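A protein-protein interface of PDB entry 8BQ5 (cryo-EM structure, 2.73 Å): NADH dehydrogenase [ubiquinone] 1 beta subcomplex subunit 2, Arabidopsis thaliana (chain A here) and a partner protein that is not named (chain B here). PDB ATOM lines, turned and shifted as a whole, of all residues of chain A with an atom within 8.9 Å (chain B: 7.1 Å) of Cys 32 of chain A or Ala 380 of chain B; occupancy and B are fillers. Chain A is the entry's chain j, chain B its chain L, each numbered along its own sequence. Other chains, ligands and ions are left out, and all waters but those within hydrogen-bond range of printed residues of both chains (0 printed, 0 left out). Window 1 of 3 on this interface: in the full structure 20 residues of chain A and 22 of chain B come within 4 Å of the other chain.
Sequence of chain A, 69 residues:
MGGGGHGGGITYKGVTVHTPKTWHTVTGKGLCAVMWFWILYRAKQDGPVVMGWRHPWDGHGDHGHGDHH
Hydrophobic or aromatic side chains of chain A within 4 Å of the printed part of chain B: His 24, Leu 31, Met 35 and Trp 38.
Of the 17 printed residues of chain B, 5 touch a printed residue of chain A.
Printed residues of chain B that touch a printed residue of chain A: Pro 376, Leu 377, Ala 380, Met 381 and Leu 475.
The backbone carbonyl oxygen (O) of His 24 of chain A is in hydrogen-bond range of the side-chain hydroxyl (OG1) of Thr 27 of chain A, at 3.3 Å.
O of Cys 32 of chain A sits close to NE1 of Trp 36 of chain A, 3.5 Å away.
The backbone carbonyl oxygen (O) of Gly 28 of chain A sits close to the side-chain sulfur (SG) of Cys 32 of chain A (3.8 Å).
Cys 32 of chain A touches just one residue of chain B: Ala 380 (3.8 Å).
Ala 380 of chain B touches just these residues of chain A: Gly 28 and Cys 32.
Of the printed residues of chain A, Met 381 of chain B touches Leu 31.
Of the printed residues of chain B, Trp 38 of chain A touches Leu 475.
Printed residues of chain B within 4 Å of Gly 28 of chain A: Ala 380 (3.6 Å).
Of the printed residues of chain A, Leu 377 of chain B touches His 24 and Thr 27.
Printed residues of chain B within 4 Å of His 24 of chain A: Pro 376 (3.8 Å) and Leu 377 (3.5 Å).
Of the printed residues of chain A, Leu 475 of chain B touches Met 35 (3.5 Å) and Trp 38 (3.3 Å).
Val 34 of chain A touches none of the printed residues of chain B.
Phe 442 of chain B touches none of the printed residues of chain A.
The nearest residue of chain B that does not touch Cys 32 of chain A is Ile 384 of chain B (4.4 Å).
The nearest printed residue of chain B that does not touch Gly 28 of chain A is Pro 376 of chain B (4.1 Å).
Among the printed residues, merely in contact across the chains: His 24 of chain A with Pro 376 of chain B (3.8 Å), His 24 of chain A with Leu 377 of chain B (3.5 Å), Thr 25 of chain A with Pro 376 of chain B (3.6 Å), Thr 27 of chain A with Leu 377 of chain B (3.8 Å), Gly 28 of chain A with Ala 380 of chain B (3.6 Å), Leu 31 of chain A with Met 381 of chain B (3.8 Å), Cys 32 of chain A with Ala 380 of chain B (3.8 Å) and Met 35 of chain A with Leu 475 of chain B (3.5 Å).
The indole nitrogen (NE1) of Trp 38 of chain A is in hydrogen-bond range of the backbone carbonyl oxygen (O) of Leu 475 of chain B, at 3.3 Å.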
ATOM      1  N   HIS A  24      27.818 -21.967  25.398  1.00  0.00           N
ATOM      2  CA  HIS A  24      26.656 -22.233  24.558  1.00  0.00           C
ATOM      3  C   HIS A  24      25.768 -21.000  24.450  1.00  0.00           C
ATOM      4  O   HIS A  24      25.179 -20.734  23.397  1.00  0.00           O
ATOM      5  CB  HIS A  24      25.880 -23.420  25.117  1.00  0.00           C
ATOM      6  CG  HIS A  24      26.364 -24.739  24.608  1.00  0.00           C
ATOM      7  ND1 HIS A  24      25.809 -25.937  24.997  1.00  0.00           N
ATOM      8  CD2 HIS A  24      27.356 -25.047  23.739  1.00  0.00           C
ATOM      9  CE1 HIS A  24      26.435 -26.928  24.389  1.00  0.00           C
ATOM     10  NE2 HIS A  24      27.378 -26.415  23.619  1.00  0.00           N
ATOM     11  N   THR A  25      25.651 -20.240  25.541  1.00  0.00           N
ATOM     12  CA  THR A  25      24.918 -18.980  25.491  1.00  0.00           C
ATOM     13  C   THR A  25      25.693 -17.936  24.698  1.00  0.00           C
ATOM     14  O   THR A  25      25.114 -17.182  23.908  1.00  0.00           O
ATOM     15  CB  THR A  25      24.640 -18.476  26.908  1.00  0.00           C
ATOM     16  OG1 THR A  25      23.907 -19.470  27.635  1.00  0.00           O
ATOM     17  CG2 THR A  25      23.831 -17.190  26.869  1.00  0.00           C
ATOM     18  N   VAL A  26      27.012 -17.882  24.897  1.00  0.00           N
ATOM     19  CA  VAL A  26      27.834 -16.887  24.215  1.00  0.00           C
ATOM     20  C   VAL A  26      27.831 -17.123  22.712  1.00  0.00           C
ATOM     21  O   VAL A  26      27.593 -16.201  21.923  1.00  0.00           O
ATOM     22  CB  VAL A  26      29.264 -16.898  24.787  1.00  0.00           C
ATOM     23  CG1 VAL A  26      30.234 -16.225  23.824  1.00  0.00           C
ATOM     24  CG2 VAL A  26      29.296 -16.217  26.146  1.00  0.00           C
ATOM     25  N   THR A  27      28.083 -18.365  22.291  1.00  0.00           N
ATOM     26  CA  THR A  27      28.170 -18.655  20.864  1.00  0.00           C
ATOM     27  C   THR A  27      26.843 -18.386  20.166  1.00  0.00           C
ATOM     28  O   THR A  27      26.817 -17.820  19.066  1.00  0.00           O
ATOM     29  CB  THR A  27      28.607 -20.103  20.648  1.00  0.00           C
ATOM     30  OG1 THR A  27      28.023 -20.932  21.660  1.00  0.00           O
ATOM     31  CG2 THR A  27      30.120 -20.213  20.725  1.00  0.00           C
ATOM     32  N   GLY A  28      25.735 -18.774  20.791  1.00  0.00           N
ATOM     33  CA  GLY A  28      24.422 -18.533  20.227  1.00  0.00           C
ATOM     34  C   GLY A  28      24.120 -17.058  20.064  1.00  0.00           C
ATOM     35  O   GLY A  28      23.604 -16.632  19.027  1.00  0.00           O
ATOM     36  N   LYS A  29      24.443 -16.267  21.089  1.00  0.00           N
ATOM     37  CA  LYS A  29      24.258 -14.823  21.003  1.00  0.00           C
ATOM     38  C   LYS A  29      25.157 -14.216  19.934  1.00  0.00           C
ATOM     39  O   LYS A  29      24.714 -13.396  19.123  1.00  0.00           O
ATOM     40  CB  LYS A  29      24.536 -14.182  22.363  1.00  0.00           C
ATOM     41  CG  LYS A  29      23.402 -14.317  23.358  1.00  0.00           C
ATOM     42  CD  LYS A  29      22.465 -13.128  23.280  1.00  0.00           C
ATOM     43  CE  LYS A  29      21.268 -13.309  24.196  1.00  0.00           C
ATOM     44  NZ  LYS A  29      20.491 -14.530  23.850  1.00  0.00           N
ATOM     45  N   GLY A  30      26.431 -14.609  19.923  1.00  0.00           N
ATOM     46  CA  GLY A  30      27.379 -13.993  19.010  1.00  0.00           C
ATOM     47  C   GLY A  30      27.074 -14.269  17.550  1.00  0.00           C
ATOM     48  O   GLY A  30      27.078 -13.353  16.725  1.00  0.00           O
ATOM     49  N   LEU A  31      26.794 -15.532  17.215  1.00  0.00           N
ATOM     50  CA  LEU A  31      26.588 -15.899  15.816  1.00  0.00           C
ATOM     51  C   LEU A  31      25.359 -15.214  15.237  1.00  0.00           C
ATOM     52  O   LEU A  31      25.375 -14.761  14.086  1.00  0.00           O
ATOM     53  CB  LEU A  31      26.475 -17.417  15.678  1.00  0.00           C
ATOM     54  CG  LEU A  31      27.761 -18.181  15.349  1.00  0.00           C
ATOM     55  CD1 LEU A  31      28.966 -17.617  16.095  1.00  0.00           C
ATOM     56  CD2 LEU A  31      27.592 -19.659  15.648  1.00  0.00           C
ATOM     57  N   CYS A  32      24.276 -15.139  16.012  1.00  0.00           N
ATOM     58  CA  CYS A  32      23.120 -14.372  15.564  1.00  0.00           C
ATOM     59  C   CYS A  32      23.466 -12.897  15.414  1.00  0.00           C
ATOM     60  O   CYS A  32      23.030 -12.254  14.453  1.00  0.00           O
ATOM     61  CB  CYS A  32      21.953 -14.556  16.532  1.00  0.00           C
ATOM     62  SG  CYS A  32      21.047 -16.105  16.314  1.00  0.00           S
ATOM     63  N   ALA A  33      24.261 -12.353  16.339  1.00  0.00           N
ATOM     64  CA  ALA A  33      24.649 -10.948  16.259  1.00  0.00           C
ATOM     65  C   ALA A  33      25.444 -10.657  14.992  1.00  0.00           C
ATOM     66  O   ALA A  33      25.231  -9.625  14.347  1.00  0.00           O
ATOM     67  CB  ALA A  33      25.452 -10.553  17.498  1.00  0.00           C
ATOM     68  N   VAL A  34      26.369 -11.549  14.623  1.00  0.00           N
ATOM     69  CA  VAL A  34      27.098 -11.380  13.369  1.00  0.00           C
ATOM     70  C   VAL A  34      26.126 -11.377  12.200  1.00  0.00           C
ATOM     71  O   VAL A  34      26.292 -10.626  11.230  1.00  0.00           O
ATOM     72  CB  VAL A  34      28.163 -12.482  13.207  1.00  0.00           C
ATOM     73  CG1 VAL A  34      28.945 -12.282  11.916  1.00  0.00           C
ATOM     74  CG2 VAL A  34      29.098 -12.512  14.402  1.00  0.00           C
ATOM     75  N   MET A  35      25.096 -12.217  12.277  1.00  0.00           N
ATOM     76  CA  MET A  35      24.092 -12.279  11.223  1.00  0.00           C
ATOM     77  C   MET A  35      23.312 -10.973  11.119  1.00  0.00           C
ATOM     78  O   MET A  35      23.068 -10.470  10.016  1.00  0.00           O
ATOM     79  CB  MET A  35      23.157 -13.458  11.483  1.00  0.00           C
ATOM     80  CG  MET A  35      21.875 -13.418  10.697  1.00  0.00           C
ATOM     81  SD  MET A  35      20.547 -14.285  11.540  1.00  0.00           S
ATOM     82  CE  MET A  35      19.231 -14.030  10.361  1.00  0.00           C
ATOM     83  N   TRP A  36      22.906 -10.407  12.261  1.00  0.00           N
ATOM     84  CA  TRP A  36      22.196  -9.130  12.230  1.00  0.00           C
ATOM     85  C   TRP A  36      23.083  -8.027  11.669  1.00  0.00           C
ATOM     86  O   TRP A  36      22.642  -7.230  10.833  1.00  0.00           O
ATOM     87  CB  TRP A  36      21.708  -8.752  13.630  1.00  0.00           C
ATOM     88  CG  TRP A  36      20.809  -9.764  14.275  1.00  0.00           C
ATOM     89  CD1 TRP A  36      21.018 -10.405  15.458  1.00  0.00           C
ATOM     90  CD2 TRP A  36      19.551 -10.238  13.780  1.00  0.00           C
ATOM     91  NE1 TRP A  36      19.978 -11.257  15.728  1.00  0.00           N
ATOM     92  CE2 TRP A  36      19.061 -11.172  14.714  1.00  0.00           C
ATOM     93  CE3 TRP A  36      18.792  -9.967  12.637  1.00  0.00           C
ATOM     94  CZ2 TRP A  36      17.850 -11.836  14.541  1.00  0.00           C
ATOM     95  CZ3 TRP A  36      17.591 -10.627  12.467  1.00  0.00           C
ATOM     96  CH2 TRP A  36      17.131 -11.549  13.415  1.00  0.00           C
ATOM     97  N   PHE A  37      24.342  -7.974  12.111  1.00  0.00           N
ATOM     98  CA  PHE A  37      25.283  -7.000  11.572  1.00  0.00           C
ATOM     99  C   PHE A  37      25.526  -7.230  10.085  1.00  0.00           C
ATOM    100  O   PHE A  37      25.724  -6.274   9.327  1.00  0.00           O
ATOM    101  CB  PHE A  37      26.595  -7.063  12.355  1.00  0.00           C
ATOM    102  CG  PHE A  37      27.646  -6.111  11.865  1.00  0.00           C
ATOM    103  CD1 PHE A  37      27.743  -4.835  12.393  1.00  0.00           C
ATOM    104  CD2 PHE A  37      28.558  -6.500  10.898  1.00  0.00           C
ATOM    105  CE1 PHE A  37      28.715  -3.962  11.952  1.00  0.00           C
ATOM    106  CE2 PHE A  37      29.528  -5.632  10.452  1.00  0.00           C
ATOM    107  CZ  PHE A  37      29.608  -4.361  10.981  1.00  0.00           C
ATOM    108  N   TRP A  38      25.530  -8.495   9.654  1.00  0.00           N
ATOM    109  CA  TRP A  38      25.661  -8.794   8.233  1.00  0.00           C
ATOM    110  C   TRP A  38      24.483  -8.244   7.440  1.00  0.00           C
ATOM    111  O   TRP A  38      24.664  -7.657   6.367  1.00  0.00           O
ATOM    112  CB  TRP A  38      25.783 -10.305   8.034  1.00  0.00           C
ATOM    113  CG  TRP A  38      25.877 -10.744   6.604  1.00  0.00           C
ATOM    114  CD1 TRP A  38      24.932 -11.425   5.896  1.00  0.00           C
ATOM    115  CD2 TRP A  38      26.984 -10.557   5.715  1.00  0.00           C
ATOM    116  NE1 TRP A  38      25.373 -11.665   4.621  1.00  0.00           N
ATOM    117  CE2 TRP A  38      26.633 -11.142   4.483  1.00  0.00           C
ATOM    118  CE3 TRP A  38      28.236  -9.947   5.838  1.00  0.00           C
ATOM    119  CZ2 TRP A  38      27.486 -11.136   3.382  1.00  0.00           C
ATOM    120  CZ3 TRP A  38      29.082  -9.943   4.744  1.00  0.00           C
ATOM    121  CH2 TRP A  38      28.704 -10.532   3.533  1.00  0.00           C
ATOM    122  N   ILE A  39      23.267  -8.417   7.959  1.00  0.00           N
ATOM    123  CA  ILE A  39      22.077  -8.006   7.220  1.00  0.00           C
ATOM    124  C   ILE A  39      21.989  -6.487   7.142  1.00  0.00           C
ATOM    125  O   ILE A  39      21.649  -5.924   6.095  1.00  0.00           O
ATOM    126  CB  ILE A  39      20.819  -8.625   7.857  1.00  0.00           C
ATOM    127  CG1 ILE A  39      20.798 -10.135   7.607  1.00  0.00           C
ATOM    128  CG2 ILE A  39      19.559  -7.985   7.306  1.00  0.00           C
ATOM    129  CD1 ILE A  39      19.777 -10.875   8.432  1.00  0.00           C
ATOM    130  N   LEU B 347      21.780 -27.908   8.505  1.00  0.00           N
ATOM    131  CA  LEU B 347      21.685 -27.164   9.785  1.00  0.00           C
ATOM    132  C   LEU B 347      20.322 -27.450  10.415  1.00  0.00           C
ATOM    133  O   LEU B 347      20.303 -27.769  11.592  1.00  0.00           O
ATOM    134  CB  LEU B 347      21.866 -25.670   9.506  1.00  0.00           C
ATOM    135  CG  LEU B 347      21.972 -24.774  10.737  1.00  0.00           C
ATOM    136  CD1 LEU B 347      23.083 -25.254  11.655  1.00  0.00           C
ATOM    137  CD2 LEU B 347      22.209 -23.330  10.329  1.00  0.00           C
ATOM    138  N   SER B 351      20.396 -29.524  13.681  1.00  0.00           N
ATOM    139  CA  SER B 351      19.927 -28.799  14.858  1.00  0.00           C
ATOM    140  C   SER B 351      18.682 -29.451  15.445  1.00  0.00           C
ATOM    141  O   SER B 351      18.544 -29.546  16.670  1.00  0.00           O
ATOM    142  CB  SER B 351      19.649 -27.339  14.508  1.00  0.00           C
ATOM    143  OG  SER B 351      20.764 -26.728  13.887  1.00  0.00           O
ATOM    144  N   ALA B 372      13.479 -21.840  24.309  1.00  0.00           N
ATOM    145  CA  ALA B 372      14.174 -20.712  23.644  1.00  0.00           C
ATOM    146  C   ALA B 372      15.336 -20.282  24.537  1.00  0.00           C
ATOM    147  O   ALA B 372      16.335 -19.777  23.998  1.00  0.00           O
ATOM    148  CB  ALA B 372      13.219 -19.582  23.435  1.00  0.00           C
ATOM    149  N   PHE B 375      17.885 -23.947  25.435  1.00  0.00           N
ATOM    150  CA  PHE B 375      18.854 -24.382  24.395  1.00  0.00           C
ATOM    151  C   PHE B 375      19.293 -23.185  23.555  1.00  0.00           C
ATOM    152  O   PHE B 375      18.788 -23.028  22.432  1.00  0.00           O
ATOM    153  CB  PHE B 375      18.255 -25.448  23.476  1.00  0.00           C
ATOM    154  CG  PHE B 375      17.793 -26.698  24.175  1.00  0.00           C
ATOM    155  CD1 PHE B 375      16.493 -27.144  24.033  1.00  0.00           C
ATOM    156  CD2 PHE B 375      18.659 -27.424  24.977  1.00  0.00           C
ATOM    157  CE1 PHE B 375      16.066 -28.296  24.673  1.00  0.00           C
ATOM    158  CE2 PHE B 375      18.228 -28.569  25.623  1.00  0.00           C
ATOM    159  CZ  PHE B 375      16.932 -28.999  25.473  1.00  0.00           C
ATOM    160  N   PRO B 376      20.225 -22.337  24.034  1.00  0.00           N
ATOM    161  CA  PRO B 376      20.600 -21.127  23.284  1.00  0.00           C
ATOM    162  C   PRO B 376      21.314 -21.432  21.982  1.00  0.00           C
ATOM    163  O   PRO B 376      21.048 -20.781  20.964  1.00  0.00           O
ATOM    164  CB  PRO B 376      21.502 -20.369  24.272  1.00  0.00           C
ATOM    165  CG  PRO B 376      21.373 -21.084  25.587  1.00  0.00           C
ATOM    166  CD  PRO B 376      21.005 -22.487  25.270  1.00  0.00           C
ATOM    167  N   LEU B 377      22.219 -22.413  21.983  1.00  0.00           N
ATOM    168  CA  LEU B 377      22.979 -22.705  20.775  1.00  0.00           C
ATOM    169  C   LEU B 377      22.103 -23.372  19.722  1.00  0.00           C
ATOM    170  O   LEU B 377      22.228 -23.084  18.527  1.00  0.00           O
ATOM    171  CB  LEU B 377      24.187 -23.578  21.111  1.00  0.00           C
ATOM    172  CG  LEU B 377      25.113 -23.912  19.941  1.00  0.00           C
ATOM    173  CD1 LEU B 377      25.597 -22.636  19.268  1.00  0.00           C
ATOM    174  CD2 LEU B 377      26.291 -24.738  20.417  1.00  0.00           C
ATOM    175  N   THR B 378      21.204 -24.260  20.147  1.00  0.00           N
ATOM    176  CA  THR B 378      20.350 -24.964  19.197  1.00  0.00           C
ATOM    177  C   THR B 378      19.297 -24.034  18.602  1.00  0.00           C
ATOM    178  O   THR B 378      19.051 -24.055  17.390  1.00  0.00           O
ATOM    179  CB  THR B 378      19.690 -26.161  19.878  1.00  0.00           C
ATOM    180  OG1 THR B 378      20.666 -27.187  20.095  1.00  0.00           O
ATOM    181  CG2 THR B 378      18.584 -26.706  19.013  1.00  0.00           C
ATOM    182  N   TYR B 379      18.668 -23.209  19.440  1.00  0.00           N
ATOM    183  CA  TYR B 379      17.691 -22.250  18.934  1.00  0.00           C
ATOM    184  C   TYR B 379      18.343 -21.259  17.981  1.00  0.00           C
ATOM    185  O   TYR B 379      17.769 -20.900  16.947  1.00  0.00           O
ATOM    186  CB  TYR B 379      17.028 -21.500  20.086  1.00  0.00           C
ATOM    187  CG  TYR B 379      16.137 -20.387  19.597  1.00  0.00           C
ATOM    188  CD1 TYR B 379      14.952 -20.670  18.939  1.00  0.00           C
ATOM    189  CD2 TYR B 379      16.503 -19.058  19.752  1.00  0.00           C
ATOM    190  CE1 TYR B 379      14.138 -19.665  18.478  1.00  0.00           C
ATOM    191  CE2 TYR B 379      15.695 -18.040  19.287  1.00  0.00           C
ATOM    192  CZ  TYR B 379      14.513 -18.352  18.652  1.00  0.00           C
ATOM    193  OH  TYR B 379      13.696 -17.351  18.184  1.00  0.00           O
ATOM    194  N   ALA B 380      19.545 -20.795  18.325  1.00  0.00           N
ATOM    195  CA  ALA B 380      20.265 -19.885  17.444  1.00  0.00           C
ATOM    196  C   ALA B 380      20.570 -20.546  16.109  1.00  0.00           C
ATOM    197  O   ALA B 380      20.503 -19.898  15.058  1.00  0.00           O
ATOM    198  CB  ALA B 380      21.552 -19.409  18.117  1.00  0.00           C
ATOM    199  N   MET B 381      20.911 -21.836  16.129  1.00  0.00           N
ATOM    200  CA  MET B 381      21.212 -22.534  14.885  1.00  0.00           C
ATOM    201  C   MET B 381      19.957 -22.754  14.049  1.00  0.00           C
ATOM    202  O   MET B 381      19.984 -22.591  12.824  1.00  0.00           O
ATOM    203  CB  MET B 381      21.908 -23.861  15.184  1.00  0.00           C
ATOM    204  CG  MET B 381      23.343 -23.796  15.762  1.00  0.00           C
ATOM    205  SD  MET B 381      24.672 -22.822  14.989  1.00  0.00           S
ATOM    206  CE  MET B 381      24.164 -21.109  15.167  1.00  0.00           C
ATOM    207  N   MET B 382      18.846 -23.124  14.689  1.00  0.00           N
ATOM    208  CA  MET B 382      17.602 -23.318  13.949  1.00  0.00           C
ATOM    209  C   MET B 382      17.059 -21.994  13.436  1.00  0.00           C
ATOM    210  O   MET B 382      16.388 -21.947  12.399  1.00  0.00           O
ATOM    211  CB  MET B 382      16.562 -24.011  14.828  1.00  0.00           C
ATOM    212  CG  MET B 382      16.882 -25.456  15.134  1.00  0.00           C
ATOM    213  SD  MET B 382      15.479 -26.567  14.952  1.00  0.00           S
ATOM    214  CE  MET B 382      15.086 -26.315  13.242  1.00  0.00           C
ATOM    215  N   LEU B 383      17.319 -20.909  14.165  1.00  0.00           N
ATOM    216  CA  LEU B 383      16.886 -19.591  13.720  1.00  0.00           C
ATOM    217  C   LEU B 383      17.588 -19.192  12.428  1.00  0.00           C
ATOM    218  O   LEU B 383      16.955 -18.688  11.494  1.00  0.00           O
ATOM    219  CB  LEU B 383      17.152 -18.564  14.819  1.00  0.00           C
ATOM    220  CG  LEU B 383      16.550 -17.173  14.639  1.00  0.00           C
ATOM    221  CD1 LEU B 383      15.192 -17.260  13.966  1.00  0.00           C
ATOM    222  CD2 LEU B 383      16.447 -16.470  15.980  1.00  0.00           C
ATOM    223  N   ILE B 384      18.903 -19.410  12.358  1.00  0.00           N
ATOM    224  CA  ILE B 384      19.659 -19.028  11.167  1.00  0.00           C
ATOM    225  C   ILE B 384      19.206 -19.847   9.966  1.00  0.00           C
ATOM    226  O   ILE B 384      18.951 -19.309   8.883  1.00  0.00           O
ATOM    227  CB  ILE B 384      21.169 -19.186  11.412  1.00  0.00           C
ATOM    228  CG1 ILE B 384      21.660 -18.176  12.448  1.00  0.00           C
ATOM    229  CG2 ILE B 384      21.939 -19.019  10.112  1.00  0.00           C
ATOM    230  CD1 ILE B 384      23.044 -18.477  12.969  1.00  0.00           C
ATOM    231  N   GLY B 385      19.096 -21.166  10.143  1.00  0.00           N
ATOM    232  CA  GLY B 385      18.731 -22.023   9.027  1.00  0.00           C
ATOM    233  C   GLY B 385      17.330 -21.759   8.514  1.00  0.00           C
ATOM    234  O   GLY B 385      17.103 -21.690   7.304  1.00  0.00           O
ATOM    235  N   PHE B 442      10.068 -23.657  20.457  1.00  0.00           N
ATOM    236  CA  PHE B 442      10.874 -22.893  21.444  1.00  0.00           C
ATOM    237  C   PHE B 442      10.209 -21.637  21.999  1.00  0.00           C
ATOM    238  O   PHE B 442      10.618 -21.227  23.087  1.00  0.00           O
ATOM    239  CB  PHE B 442      12.160 -22.394  20.785  1.00  0.00           C
ATOM    240  CG  PHE B 442      12.926 -23.385  19.946  1.00  0.00           C
ATOM    241  CD1 PHE B 442      13.857 -24.231  20.524  1.00  0.00           C
ATOM    242  CD2 PHE B 442      12.755 -23.432  18.571  1.00  0.00           C
ATOM    243  CE1 PHE B 442      14.575 -25.127  19.749  1.00  0.00           C
ATOM    244  CE2 PHE B 442      13.475 -24.328  17.798  1.00  0.00           C
ATOM    245  CZ  PHE B 442      14.383 -25.174  18.389  1.00  0.00           C
ATOM    246  N   ALA B 471      26.189 -22.988  10.228  1.00  0.00           N
ATOM    247  CA  ALA B 471      25.629 -21.652  10.399  1.00  0.00           C
ATOM    248  C   ALA B 471      26.428 -20.617   9.620  1.00  0.00           C
ATOM    249  O   ALA B 471      25.852 -19.736   8.972  1.00  0.00           O
ATOM    250  CB  ALA B 471      25.582 -21.287  11.880  1.00  0.00           C
ATOM    251  N   LEU B 475      25.249 -18.175   6.189  1.00  0.00           N
ATOM    252  CA  LEU B 475      25.215 -16.721   6.255  1.00  0.00           C
ATOM    253  C   LEU B 475      26.025 -16.074   5.140  1.00  0.00           C
ATOM    254  O   LEU B 475      25.705 -14.963   4.706  1.00  0.00           O
ATOM    255  CB  LEU B 475      25.738 -16.245   7.613  1.00  0.00           C
ATOM    256  CG  LEU B 475      24.887 -16.615   8.827  1.00  0.00           C
ATOM    257  CD1 LEU B 475      25.629 -16.348  10.124  1.00  0.00           C
ATOM    258  CD2 LEU B 475      23.590 -15.844   8.789  1.00  0.00           C
